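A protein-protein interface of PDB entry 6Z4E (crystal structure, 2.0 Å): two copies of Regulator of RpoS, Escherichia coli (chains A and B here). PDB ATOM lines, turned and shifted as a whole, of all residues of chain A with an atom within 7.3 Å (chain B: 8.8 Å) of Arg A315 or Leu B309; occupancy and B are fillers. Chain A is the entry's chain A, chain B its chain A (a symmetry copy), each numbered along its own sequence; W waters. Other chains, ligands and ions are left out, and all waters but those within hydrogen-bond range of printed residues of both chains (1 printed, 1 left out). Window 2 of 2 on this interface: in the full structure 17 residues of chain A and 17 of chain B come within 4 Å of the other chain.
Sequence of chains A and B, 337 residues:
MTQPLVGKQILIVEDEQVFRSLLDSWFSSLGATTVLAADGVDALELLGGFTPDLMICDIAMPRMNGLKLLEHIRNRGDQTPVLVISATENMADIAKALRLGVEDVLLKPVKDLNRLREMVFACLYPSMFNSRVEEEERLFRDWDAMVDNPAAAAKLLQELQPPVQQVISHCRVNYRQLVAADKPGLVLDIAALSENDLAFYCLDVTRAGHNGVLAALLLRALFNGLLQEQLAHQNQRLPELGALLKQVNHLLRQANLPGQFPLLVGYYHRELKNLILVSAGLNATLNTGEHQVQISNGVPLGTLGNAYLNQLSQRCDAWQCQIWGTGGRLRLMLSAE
Of the printed residues of chain B, Arg A315 touches Leu B309 (3.3 Å). Of the printed residues of chain A, Leu B309 touches Ser A313 and Arg A315. Gln A314 touches just one residue of chain B: Asn B310. Printed residues of chain B within 4 Å of Leu A312: Gln B311 (3.5 Å). Printed residues of chain B within 4 Å of Ser A313: Leu B309, Asn B310 and Gln B311. Of the printed residues of chain A, Val B299 touches Glu A290 (3.8 Å). Printed residues of chain B within 4 Å of His A291: Asn B297 and Asn B310. Glu B240 touches none of the printed residues of chain A. Gly B242 touches none of the printed residues of chain A. The nearest printed residue of chain B that does not touch Arg A315 is Asn B310 (5.0 Å). The nearest printed residue of chain A that does not touch Leu B309 is Gln A314 (4.3 Å). The nearest printed residue of chain B that does not touch Glu A290 is Asn B310 (5.2 Å).
Position printed for both chains: 312. Of the 10 pairs that touch across the chains among the printed residues, none has its exchanged pair printed and touching as well.
O of Gln A314 lies within hydrogen-bond range of N of Leu A275 (2.8 Å). OG1 of Thr A288 sits at hydrogen-bond distance from N of His A291 (3.3 Å). A ring nitrogen (ND1) of His A291 is in hydrogen-bond range of the side-chain amide oxygen (OE1) of Gln A314 (2.7 Å). ND2 of Asn B310 lies within hydrogen-bond range of O of Ser B279, at 2.6 Å. The side-chain amide oxygen (OD1) of Asn B297 is in hydrogen-bond range of the backbone NH (N) of Val B299 (2.7 Å). ND2 of Asn B297 sits close to ND2 of Asn B310 (3.3 Å).
The backbone carbonyl oxygen (O) of Ser A313 sits at hydrogen-bond distance from the backbone NH (N) of Gln B311.
Printed residues of chain B that touch a printed residue of chain A: Asn B297, Val B299, Leu B309, Asn B310 and Gln B311. Of the 17 printed residues of chain A, 6 touch a printed residue of chain B. Printed residues of chain A that touch a printed residue of chain B: Glu A290, His A291, Leu A312, Ser A313, Gln A314 and Arg A315. Hydrophobic or aromatic side chains of chain A within 4 Å of the printed part of chain B: His A291 and Leu A312. Among the printed residues, 10 pairs touch across the chains.
Water W1 bridges O of Gln B311 (3.1 Å) and OG of Ser A313 (3.3 Å).
Asn B297 touches Glu A290. Glu A290 touches Val B299 (CB to CG2, 3.8 Å). Asn B297 touches His A291. CG of Asn B310 touches NE2 of His A291, 3.4 Å away. Gln B311 touches Leu A312. Ser A313 touches Leu B309 (O to O, 3.6 Å). Asn B310 touches Ser A313 (CA to O, 3.4 Å). OE1 of Gln A314 touches CB of Asn B310 (3.4 Å). CD2 of Leu B309 touches NH1 of Arg A315, at 3.3 Å.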
ATOM      1  N   TYR A 268     -32.671  13.106 -28.805  1.00  0.00           N
ATOM      2  CA  TYR A 268     -32.948  14.360 -28.120  1.00  0.00           C
ATOM      3  C   TYR A 268     -33.162  14.117 -26.634  1.00  0.00           C
ATOM      4  O   TYR A 268     -33.843  13.166 -26.238  1.00  0.00           O
ATOM      5  CB  TYR A 268     -34.164  15.072 -28.714  1.00  0.00           C
ATOM      6  CG  TYR A 268     -34.395  16.431 -28.105  1.00  0.00           C
ATOM      7  CD1 TYR A 268     -33.599  17.518 -28.459  1.00  0.00           C
ATOM      8  CD2 TYR A 268     -35.395  16.629 -27.164  1.00  0.00           C
ATOM      9  CE1 TYR A 268     -33.804  18.766 -27.891  1.00  0.00           C
ATOM     10  CE2 TYR A 268     -35.608  17.864 -26.595  1.00  0.00           C
ATOM     11  CZ  TYR A 268     -34.813  18.930 -26.963  1.00  0.00           C
ATOM     12  OH  TYR A 268     -35.032  20.161 -26.393  1.00  0.00           O
ATOM     13  N   GLU A 271     -33.927  17.557 -20.934  1.00  0.00           N
ATOM     14  CA  GLU A 271     -33.347  18.390 -19.886  1.00  0.00           C
ATOM     15  C   GLU A 271     -32.057  19.051 -20.358  1.00  0.00           C
ATOM     16  O   GLU A 271     -31.867  20.257 -20.173  1.00  0.00           O
ATOM     17  CB  GLU A 271     -33.095  17.561 -18.629  1.00  0.00           C
ATOM     18  CG  GLU A 271     -34.302  17.422 -17.721  1.00  0.00           C
ATOM     19  CD  GLU A 271     -34.128  16.323 -16.693  1.00  0.00           C
ATOM     20  OE1 GLU A 271     -33.078  15.645 -16.718  1.00  0.00           O
ATOM     21  OE2 GLU A 271     -35.035  16.146 -15.850  1.00  0.00           O
ATOM     22  N   LEU A 272     -31.161  18.274 -20.971  1.00  0.00           N
ATOM     23  CA  LEU A 272     -29.932  18.833 -21.523  1.00  0.00           C
ATOM     24  C   LEU A 272     -30.188  19.684 -22.760  1.00  0.00           C
ATOM     25  O   LEU A 272     -29.332  20.498 -23.121  1.00  0.00           O
ATOM     26  CB  LEU A 272     -28.950  17.708 -21.859  1.00  0.00           C
ATOM     27  CG  LEU A 272     -28.538  16.797 -20.700  1.00  0.00           C
ATOM     28  CD1 LEU A 272     -27.793  15.575 -21.213  1.00  0.00           C
ATOM     29  CD2 LEU A 272     -27.691  17.561 -19.693  1.00  0.00           C
ATOM     30  N   LYS A 273     -31.343  19.511 -23.407  1.00  0.00           N
ATOM     31  CA  LYS A 273     -31.733  20.254 -24.608  1.00  0.00           C
ATOM     32  C   LYS A 273     -30.792  19.981 -25.777  1.00  0.00           C
ATOM     33  O   LYS A 273     -30.606  20.835 -26.646  1.00  0.00           O
ATOM     34  CB  LYS A 273     -31.826  21.760 -24.335  1.00  0.00           C
ATOM     35  CG  LYS A 273     -32.641  22.127 -23.097  1.00  0.00           C
ATOM     36  CD  LYS A 273     -34.136  22.060 -23.362  1.00  0.00           C
ATOM     37  CE  LYS A 273     -34.939  22.405 -22.111  1.00  0.00           C
ATOM     38  NZ  LYS A 273     -34.523  23.705 -21.516  1.00  0.00           N
ATOM     39  N   ASN A 274     -30.218  18.784 -25.828  1.00  0.00           N
ATOM     40  CA  ASN A 274     -29.244  18.417 -26.849  1.00  0.00           C
ATOM     41  C   ASN A 274     -29.915  17.566 -27.923  1.00  0.00           C
ATOM     42  O   ASN A 274     -30.512  16.528 -27.616  1.00  0.00           O
ATOM     43  CB  ASN A 274     -28.070  17.666 -26.222  1.00  0.00           C
ATOM     44  CG  ASN A 274     -26.947  17.417 -27.206  1.00  0.00           C
ATOM     45  OD1 ASN A 274     -26.765  18.172 -28.163  1.00  0.00           O
ATOM     46  ND2 ASN A 274     -26.180  16.360 -26.971  1.00  0.00           N
ATOM     47  N   LEU A 275     -29.816  18.009 -29.176  1.00  0.00           N
ATOM     48  CA  LEU A 275     -30.249  17.243 -30.337  1.00  0.00           C
ATOM     49  C   LEU A 275     -29.024  16.743 -31.090  1.00  0.00           C
ATOM     50  O   LEU A 275     -28.103  17.520 -31.371  1.00  0.00           O
ATOM     51  CB  LEU A 275     -31.120  18.088 -31.270  1.00  0.00           C
ATOM     52  CG  LEU A 275     -31.519  17.440 -32.600  1.00  0.00           C
ATOM     53  CD1 LEU A 275     -32.495  16.287 -32.368  1.00  0.00           C
ATOM     54  CD2 LEU A 275     -32.120  18.464 -33.545  1.00  0.00           C
ATOM     55  N   THR A 288     -33.760  25.675 -35.822  1.00  0.00           N
ATOM     56  CA  THR A 288     -33.971  25.914 -34.398  1.00  0.00           C
ATOM     57  C   THR A 288     -34.249  27.380 -34.084  1.00  0.00           C
ATOM     58  O   THR A 288     -34.279  27.755 -32.907  1.00  0.00           O
ATOM     59  CB  THR A 288     -32.764  25.440 -33.583  1.00  0.00           C
ATOM     60  OG1 THR A 288     -31.666  26.339 -33.790  1.00  0.00           O
ATOM     61  CG2 THR A 288     -32.354  24.036 -33.997  1.00  0.00           C
ATOM     62  N   GLU A 290     -32.434  30.220 -34.066  1.00  0.00           N
ATOM     63  CA  GLU A 290     -31.113  30.832 -34.150  1.00  0.00           C
ATOM     64  C   GLU A 290     -30.194  30.127 -35.141  1.00  0.00           C
ATOM     65  O   GLU A 290     -29.220  30.731 -35.604  1.00  0.00           O
ATOM     66  CB  GLU A 290     -30.457  30.836 -32.767  1.00  0.00           C
ATOM     67  CG  GLU A 290     -30.076  29.441 -32.277  1.00  0.00           C
ATOM     68  CD  GLU A 290     -28.897  29.445 -31.324  1.00  0.00           C
ATOM     69  OE1 GLU A 290     -27.783  29.080 -31.757  1.00  0.00           O
ATOM     70  OE2 GLU A 290     -29.086  29.793 -30.139  1.00  0.00           O
ATOM     71  N   HIS A 291     -30.479  28.873 -35.480  1.00  0.00           N
ATOM     72  CA  HIS A 291     -29.568  28.045 -36.255  1.00  0.00           C
ATOM     73  C   HIS A 291     -30.340  27.308 -37.338  1.00  0.00           C
ATOM     74  O   HIS A 291     -31.465  26.854 -37.109  1.00  0.00           O
ATOM     75  CB  HIS A 291     -28.840  27.047 -35.340  1.00  0.00           C
ATOM     76  CG  HIS A 291     -27.534  26.559 -35.884  1.00  0.00           C
ATOM     77  ND1 HIS A 291     -27.334  25.255 -36.285  1.00  0.00           N
ATOM     78  CD2 HIS A 291     -26.359  27.199 -36.092  1.00  0.00           C
ATOM     79  CE1 HIS A 291     -26.092  25.113 -36.714  1.00  0.00           C
ATOM     80  NE2 HIS A 291     -25.481  26.279 -36.612  1.00  0.00           N
ATOM     81  N   LEU A 312     -24.275  16.007 -36.463  1.00  0.00           N
ATOM     82  CA  LEU A 312     -24.708  17.355 -36.139  1.00  0.00           C
ATOM     83  C   LEU A 312     -25.212  17.335 -34.706  1.00  0.00           C
ATOM     84  O   LEU A 312     -26.099  16.542 -34.372  1.00  0.00           O
ATOM     85  CB  LEU A 312     -25.803  17.814 -37.103  1.00  0.00           C
ATOM     86  CG  LEU A 312     -26.706  18.968 -36.672  1.00  0.00           C
ATOM     87  CD1 LEU A 312     -25.897  20.226 -36.367  1.00  0.00           C
ATOM     88  CD2 LEU A 312     -27.747  19.240 -37.739  1.00  0.00           C
ATOM     89  N   SER A 313     -24.630  18.174 -33.856  1.00  0.00           N
ATOM     90  CA  SER A 313     -25.100  18.336 -32.488  1.00  0.00           C
ATOM     91  C   SER A 313     -25.532  19.779 -32.292  1.00  0.00           C
ATOM     92  O   SER A 313     -24.821  20.707 -32.689  1.00  0.00           O
ATOM     93  CB  SER A 313     -24.023  17.938 -31.476  1.00  0.00           C
ATOM     94  OG  SER A 313     -22.921  18.819 -31.532  1.00  0.00           O
ATOM     95  N   GLN A 314     -26.703  19.967 -31.697  1.00  0.00           N
ATOM     96  CA  GLN A 314     -27.256  21.304 -31.557  1.00  0.00           C
ATOM     97  C   GLN A 314     -28.042  21.371 -30.259  1.00  0.00           C
ATOM     98  O   GLN A 314     -28.796  20.448 -29.942  1.00  0.00           O
ATOM     99  CB  GLN A 314     -28.151  21.644 -32.753  1.00  0.00           C
ATOM    100  CG  GLN A 314     -29.077  22.821 -32.532  1.00  0.00           C
ATOM    101  CD  GLN A 314     -28.377  24.150 -32.734  1.00  0.00           C
ATOM    102  OE1 GLN A 314     -27.700  24.362 -33.740  1.00  0.00           O
ATOM    103  NE2 GLN A 314     -28.537  25.055 -31.774  1.00  0.00           N
ATOM    104  N   ARG A 315     -27.856  22.446 -29.502  1.00  0.00           N
ATOM    105  CA  ARG A 315     -28.623  22.670 -28.286  1.00  0.00           C
ATOM    106  C   ARG A 315     -29.779  23.610 -28.604  1.00  0.00           C
ATOM    107  O   ARG A 315     -29.568  24.711 -29.123  1.00  0.00           O
ATOM    108  CB  ARG A 315     -27.753  23.236 -27.166  1.00  0.00           C
ATOM    109  CG  ARG A 315     -28.313  22.947 -25.782  1.00  0.00           C
ATOM    110  CD  ARG A 315     -27.370  23.410 -24.695  1.00  0.00           C
ATOM    111  NE  ARG A 315     -27.086  22.361 -23.718  1.00  0.00           N
ATOM    112  CZ  ARG A 315     -26.233  21.362 -23.921  1.00  0.00           C
ATOM    113  NH1 ARG A 315     -25.584  21.269 -25.073  1.00  0.00           N
ATOM    114  NH2 ARG A 315     -26.030  20.454 -22.977  1.00  0.00           N
ATOM    115  N   CYS A 316     -30.995  23.169 -28.294  1.00  0.00           N
ATOM    116  CA  CYS A 316     -32.194  23.915 -28.645  1.00  0.00           C
ATOM    117  C   CYS A 316     -33.335  23.466 -27.748  1.00  0.00           C
ATOM    118  O   CYS A 316     -33.367  22.323 -27.286  1.00  0.00           O
ATOM    119  CB  CYS A 316     -32.578  23.701 -30.117  1.00  0.00           C
ATOM    120  SG  CYS A 316     -32.393  21.987 -30.698  1.00  0.00           S
ATOM    121  N   ASP A 317     -34.274  24.382 -27.517  1.00  0.00           N
ATOM    122  CA  ASP A 317     -35.501  24.057 -26.804  1.00  0.00           C
ATOM    123  C   ASP A 317     -36.586  23.549 -27.737  1.00  0.00           C
ATOM    124  O   ASP A 317     -37.466  22.794 -27.305  1.00  0.00           O
ATOM    125  CB  ASP A 317     -36.012  25.285 -26.046  1.00  0.00           C
ATOM    126  CG  ASP A 317     -34.966  25.872 -25.124  1.00  0.00           C
ATOM    127  OD1 ASP A 317     -34.152  25.094 -24.583  1.00  0.00           O
ATOM    128  OD2 ASP A 317     -34.961  27.108 -24.935  1.00  0.00           O
ATOM    129  N   ALA A 318     -36.539  23.947 -29.005  1.00  0.00           N
ATOM    130  CA  ALA A 318     -37.506  23.508 -29.999  1.00  0.00           C
ATOM    131  C   ALA A 318     -36.793  23.401 -31.336  1.00  0.00           C
ATOM    132  O   ALA A 318     -35.778  24.064 -31.563  1.00  0.00           O
ATOM    133  CB  ALA A 318     -38.694  24.472 -30.100  1.00  0.00           C
ATOM    134  N   TRP A 319     -37.320  22.555 -32.218  1.00  0.00           N
ATOM    135  CA  TRP A 319     -36.724  22.444 -33.539  1.00  0.00           C
ATOM    136  C   TRP A 319     -37.752  21.908 -34.517  1.00  0.00           C
ATOM    137  O   TRP A 319     -38.740  21.280 -34.132  1.00  0.00           O
ATOM    138  CB  TRP A 319     -35.472  21.556 -33.538  1.00  0.00           C
ATOM    139  CG  TRP A 319     -35.592  20.237 -32.810  1.00  0.00           C
ATOM    140  CD1 TRP A 319     -35.273  19.988 -31.504  1.00  0.00           C
ATOM    141  CD2 TRP A 319     -36.032  18.986 -33.358  1.00  0.00           C
ATOM    142  NE1 TRP A 319     -35.491  18.662 -31.208  1.00  0.00           N
ATOM    143  CE2 TRP A 319     -35.960  18.028 -32.328  1.00  0.00           C
ATOM    144  CE3 TRP A 319     -36.485  18.586 -34.620  1.00  0.00           C
ATOM    145  CZ2 TRP A 319     -36.323  16.696 -32.518  1.00  0.00           C
ATOM    146  CZ3 TRP A 319     -36.847  17.265 -34.806  1.00  0.00           C
ATOM    147  CH2 TRP A 319     -36.764  16.336 -33.762  1.00  0.00           C
ATOM    148  N   GLU B 240     -12.840  21.033 -27.447  1.00  0.00           N
ATOM    149  CA  GLU B 240     -14.166  21.548 -27.112  1.00  0.00           C
ATOM    150  C   GLU B 240     -14.252  22.960 -27.676  1.00  0.00           C
ATOM    151  O   GLU B 240     -14.017  23.941 -26.970  1.00  0.00           O
ATOM    152  CB  GLU B 240     -14.408  21.524 -25.600  1.00  0.00           C
ATOM    153  CG  GLU B 240     -14.569  20.131 -25.021  1.00  0.00           C
ATOM    154  CD  GLU B 240     -15.817  19.426 -25.524  1.00  0.00           C
ATOM    155  OE1 GLU B 240     -16.763  20.117 -25.959  1.00  0.00           O
ATOM    156  OE2 GLU B 240     -15.848  18.178 -25.489  1.00  0.00           O
ATOM    157  N   LEU B 241     -14.589  23.058 -28.964  1.00  0.00           N
ATOM    158  CA  LEU B 241     -14.596  24.358 -29.625  1.00  0.00           C
ATOM    159  C   LEU B 241     -15.662  25.281 -29.049  1.00  0.00           C
ATOM    160  O   LEU B 241     -15.456  26.499 -28.990  1.00  0.00           O
ATOM    161  CB  LEU B 241     -14.792  24.174 -31.129  1.00  0.00           C
ATOM    162  CG  LEU B 241     -13.625  23.500 -31.859  1.00  0.00           C
ATOM    163  CD1 LEU B 241     -13.884  23.462 -33.355  1.00  0.00           C
ATOM    164  CD2 LEU B 241     -12.306  24.217 -31.564  1.00  0.00           C
ATOM    165  N   GLY B 242     -16.798  24.729 -28.616  1.00  0.00           N
ATOM    166  CA  GLY B 242     -17.800  25.552 -27.954  1.00  0.00           C
ATOM    167  C   GLY B 242     -17.271  26.210 -26.695  1.00  0.00           C
ATOM    168  O   GLY B 242     -17.491  27.402 -26.466  1.00  0.00           O
ATOM    169  N   ALA B 243     -16.552  25.445 -25.868  1.00  0.00           N
ATOM    170  CA  ALA B 243     -15.919  26.019 -24.686  1.00  0.00           C
ATOM    171  C   ALA B 243     -14.882  27.069 -25.068  1.00  0.00           C
ATOM    172  O   ALA B 243     -14.731  28.083 -24.382  1.00  0.00           O
ATOM    173  CB  ALA B 243     -15.281  24.913 -23.845  1.00  0.00           C
ATOM    174  N   LEU B 245     -14.990  29.065 -27.655  1.00  0.00           N
ATOM    175  CA  LEU B 245     -15.719  30.272 -28.028  1.00  0.00           C
ATOM    176  C   LEU B 245     -16.174  31.045 -26.798  1.00  0.00           C
ATOM    177  O   LEU B 245     -16.127  32.282 -26.783  1.00  0.00           O
ATOM    178  CB  LEU B 245     -16.912  29.913 -28.909  1.00  0.00           C
ATOM    179  CG  LEU B 245     -16.581  29.552 -30.358  1.00  0.00           C
ATOM    180  CD1 LEU B 245     -17.848  29.181 -31.106  1.00  0.00           C
ATOM    181  CD2 LEU B 245     -15.878  30.702 -31.050  1.00  0.00           C
ATOM    182  N   LYS B 246     -16.629  30.336 -25.756  1.00  0.00           N
ATOM    183  CA  LYS B 246     -16.948  31.001 -24.498  1.00  0.00           C
ATOM    184  C   LYS B 246     -15.732  31.737 -23.948  1.00  0.00           C
ATOM    185  O   LYS B 246     -15.846  32.866 -23.454  1.00  0.00           O
ATOM    186  CB  LYS B 246     -17.469  29.979 -23.483  1.00  0.00           C
ATOM    187  CG  LYS B 246     -17.485  30.462 -22.031  1.00  0.00           C
ATOM    188  CD  LYS B 246     -16.978  29.388 -21.059  1.00  0.00           C
ATOM    189  CE  LYS B 246     -15.748  28.664 -21.610  1.00  0.00           C
ATOM    190  NZ  LYS B 246     -14.979  27.886 -20.596  1.00  0.00           N
ATOM    191  N   LEU B 277     -16.460  21.655 -36.750  1.00  0.00           N
ATOM    192  CA  LEU B 277     -16.780  23.040 -37.071  1.00  0.00           C
ATOM    193  C   LEU B 277     -17.829  23.562 -36.104  1.00  0.00           C
ATOM    194  O   LEU B 277     -18.804  22.870 -35.802  1.00  0.00           O
ATOM    195  CB  LEU B 277     -17.307  23.188 -38.501  1.00  0.00           C
ATOM    196  CG  LEU B 277     -16.370  22.877 -39.661  1.00  0.00           C
ATOM    197  CD1 LEU B 277     -17.130  23.004 -40.975  1.00  0.00           C
ATOM    198  CD2 LEU B 277     -15.167  23.793 -39.638  1.00  0.00           C
ATOM    199  N   VAL B 278     -17.631  24.789 -35.630  1.00  0.00           N
ATOM    200  CA  VAL B 278     -18.623  25.491 -34.822  1.00  0.00           C
ATOM    201  C   VAL B 278     -18.727  26.915 -35.345  1.00  0.00           C
ATOM    202  O   VAL B 278     -17.712  27.608 -35.479  1.00  0.00           O
ATOM    203  CB  VAL B 278     -18.260  25.493 -33.323  1.00  0.00           C
ATOM    204  CG1 VAL B 278     -19.299  26.270 -32.529  1.00  0.00           C
ATOM    205  CG2 VAL B 278     -18.132  24.075 -32.794  1.00  0.00           C
ATOM    206  N   SER B 279     -19.944  27.357 -35.642  1.00  0.00           N
ATOM    207  CA  SER B 279     -20.174  28.705 -36.136  1.00  0.00           C
ATOM    208  C   SER B 279     -20.944  29.518 -35.109  1.00  0.00           C
ATOM    209  O   SER B 279     -21.905  29.029 -34.505  1.00  0.00           O
ATOM    210  CB  SER B 279     -20.944  28.701 -37.455  1.00  0.00           C
ATOM    211  OG  SER B 279     -21.312  30.031 -37.792  1.00  0.00           O
ATOM    212  N   ALA B 280     -20.513  30.766 -34.917  1.00  0.00           N
ATOM    213  CA  ALA B 280     -21.213  31.735 -34.076  1.00  0.00           C
ATOM    214  C   ALA B 280     -21.460  32.980 -34.925  1.00  0.00           C
ATOM    215  O   ALA B 280     -20.695  33.946 -34.874  1.00  0.00           O
ATOM    216  CB  ALA B 280     -20.418  32.049 -32.816  1.00  0.00           C
ATOM    217  N   ASN B 297     -25.551  30.226 -38.834  1.00  0.00           N
ATOM    218  CA  ASN B 297     -25.795  30.597 -37.449  1.00  0.00           C
ATOM    219  C   ASN B 297     -26.018  32.098 -37.351  1.00  0.00           C
ATOM    220  O   ASN B 297     -25.339  32.882 -38.018  1.00  0.00           O
ATOM    221  CB  ASN B 297     -24.624  30.186 -36.550  1.00  0.00           C
ATOM    222  CG  ASN B 297     -24.880  30.500 -35.082  1.00  0.00           C
ATOM    223  OD1 ASN B 297     -24.607  31.607 -34.616  1.00  0.00           O
ATOM    224  ND2 ASN B 297     -25.405  29.525 -34.349  1.00  0.00           N
ATOM    225  N   VAL B 299     -26.094  33.845 -34.217  1.00  0.00           N
ATOM    226  CA  VAL B 299     -25.695  34.393 -32.923  1.00  0.00           C
ATOM    227  C   VAL B 299     -24.196  34.659 -32.929  1.00  0.00           C
ATOM    228  O   VAL B 299     -23.406  33.772 -32.572  1.00  0.00           O
ATOM    229  CB  VAL B 299     -26.084  33.456 -31.769  1.00  0.00           C
ATOM    230  CG1 VAL B 299     -25.805  34.130 -30.432  1.00  0.00           C
ATOM    231  CG2 VAL B 299     -27.554  33.061 -31.875  1.00  0.00           C
ATOM    232  N   GLY B 305     -24.410  36.499 -22.324  1.00  0.00           N
ATOM    233  CA  GLY B 305     -24.692  35.154 -21.863  1.00  0.00           C
ATOM    234  C   GLY B 305     -25.183  34.179 -22.913  1.00  0.00           C
ATOM    235  O   GLY B 305     -26.159  33.460 -22.682  1.00  0.00           O
ATOM    236  N   ASN B 306     -24.519  34.133 -24.064  1.00  0.00           N
ATOM    237  CA  ASN B 306     -24.809  33.139 -25.087  1.00  0.00           C
ATOM    238  C   ASN B 306     -23.817  31.992 -24.981  1.00  0.00           C
ATOM    239  O   ASN B 306     -22.602  32.214 -24.984  1.00  0.00           O
ATOM    240  CB  ASN B 306     -24.751  33.738 -26.492  1.00  0.00           C
ATOM    241  CG  ASN B 306     -25.818  34.780 -26.729  1.00  0.00           C
ATOM    242  OD1 ASN B 306     -25.621  35.719 -27.498  1.00  0.00           O
ATOM    243  ND2 ASN B 306     -26.956  34.624 -26.067  1.00  0.00           N
ATOM    244  N   ALA B 307     -24.334  30.774 -24.879  1.00  0.00           N
ATOM    245  CA  ALA B 307     -23.519  29.586 -25.059  1.00  0.00           C
ATOM    246  C   ALA B 307     -23.625  29.139 -26.511  1.00  0.00           C
ATOM    247  O   ALA B 307     -24.709  29.156 -27.100  1.00  0.00           O
ATOM    248  CB  ALA B 307     -23.960  28.472 -24.110  1.00  0.00           C
ATOM    249  N   TYR B 308     -22.491  28.765 -27.090  1.00  0.00           N
ATOM    250  CA  TYR B 308     -22.382  28.475 -28.519  1.00  0.00           C
ATOM    251  C   TYR B 308     -22.136  26.976 -28.668  1.00  0.00           C
ATOM    252  O   TYR B 308     -20.994  26.516 -28.577  1.00  0.00           O
ATOM    253  CB  TYR B 308     -21.256  29.301 -29.144  1.00  0.00           C
ATOM    254  CG  TYR B 308     -21.242  30.753 -28.703  1.00  0.00           C
ATOM    255  CD1 TYR B 308     -22.012  31.706 -29.359  1.00  0.00           C
ATOM    256  CD2 TYR B 308     -20.464  31.168 -27.625  1.00  0.00           C
ATOM    257  CE1 TYR B 308     -22.007  33.032 -28.959  1.00  0.00           C
ATOM    258  CE2 TYR B 308     -20.451  32.493 -27.218  1.00  0.00           C
ATOM    259  CZ  TYR B 308     -21.226  33.421 -27.887  1.00  0.00           C
ATOM    260  OH  TYR B 308     -21.219  34.741 -27.487  1.00  0.00           O
ATOM    261  N   LEU B 309     -23.205  26.212 -28.907  1.00  0.00           N
ATOM    262  CA  LEU B 309     -23.119  24.762 -28.805  1.00  0.00           C
ATOM    263  C   LEU B 309     -23.452  24.007 -30.088  1.00  0.00           C
ATOM    264  O   LEU B 309     -23.463  22.769 -30.064  1.00  0.00           O
ATOM    265  CB  LEU B 309     -24.031  24.254 -27.683  1.00  0.00           C
ATOM    266  CG  LEU B 309     -23.958  25.031 -26.372  1.00  0.00           C
ATOM    267  CD1 LEU B 309     -25.102  26.052 -26.317  1.00  0.00           C
ATOM    268  CD2 LEU B 309     -23.923  24.106 -25.158  1.00  0.00           C
ATOM    269  N   ASN B 310     -23.733  24.690 -31.194  1.00  0.00           N
ATOM    270  CA  ASN B 310     -23.844  23.980 -32.461  1.00  0.00           C
ATOM    271  C   ASN B 310     -22.492  23.378 -32.825  1.00  0.00           C
ATOM    272  O   ASN B 310     -21.442  23.990 -32.611  1.00  0.00           O
ATOM    273  CB  ASN B 310     -24.337  24.913 -33.571  1.00  0.00           C
ATOM    274  CG  ASN B 310     -23.268  25.883 -34.047  1.00  0.00           C
ATOM    275  OD1 ASN B 310     -22.418  25.539 -34.872  1.00  0.00           O
ATOM    276  ND2 ASN B 310     -23.308  27.105 -33.527  1.00  0.00           N
ATOM    277  N   GLN B 311     -22.513  22.157 -33.345  1.00  0.00           N
ATOM    278  CA  GLN B 311     -21.268  21.492 -33.693  1.00  0.00           C
ATOM    279  C   GLN B 311     -21.521  20.531 -34.839  1.00  0.00           C
ATOM    280  O   GLN B 311     -22.459  19.730 -34.795  1.00  0.00           O
ATOM    281  CB  GLN B 311     -20.672  20.747 -32.494  1.00  0.00           C
ATOM    282  CG  GLN B 311     -19.278  20.196 -32.748  1.00  0.00           C
ATOM    283  CD  GLN B 311     -18.481  20.002 -31.473  1.00  0.00           C
ATOM    284  OE1 GLN B 311     -18.332  20.925 -30.676  1.00  0.00           O
ATOM    285  NE2 GLN B 311     -17.971  18.793 -31.272  1.00  0.00           N
ATOM    286  N   LEU B 312     -20.691  20.635 -35.863  1.00  0.00           N
ATOM    287  CA  LEU B 312     -20.665  19.704 -36.978  1.00  0.00           C
ATOM    288  C   LEU B 312     -19.371  18.914 -36.873  1.00  0.00           C
ATOM    289  O   LEU B 312     -18.286  19.505 -36.823  1.00  0.00           O
ATOM    290  CB  LEU B 312     -20.748  20.454 -38.307  1.00  0.00           C
ATOM    291  CG  LEU B 312     -20.271  19.738 -39.570  1.00  0.00           C
ATOM    292  CD1 LEU B 312     -21.042  18.441 -39.801  1.00  0.00           C
ATOM    293  CD2 LEU B 312     -20.393  20.660 -40.768  1.00  0.00           C
HETATM  294  O   HOH W   1     -21.269  17.074 -33.801  1.00  0.00           O
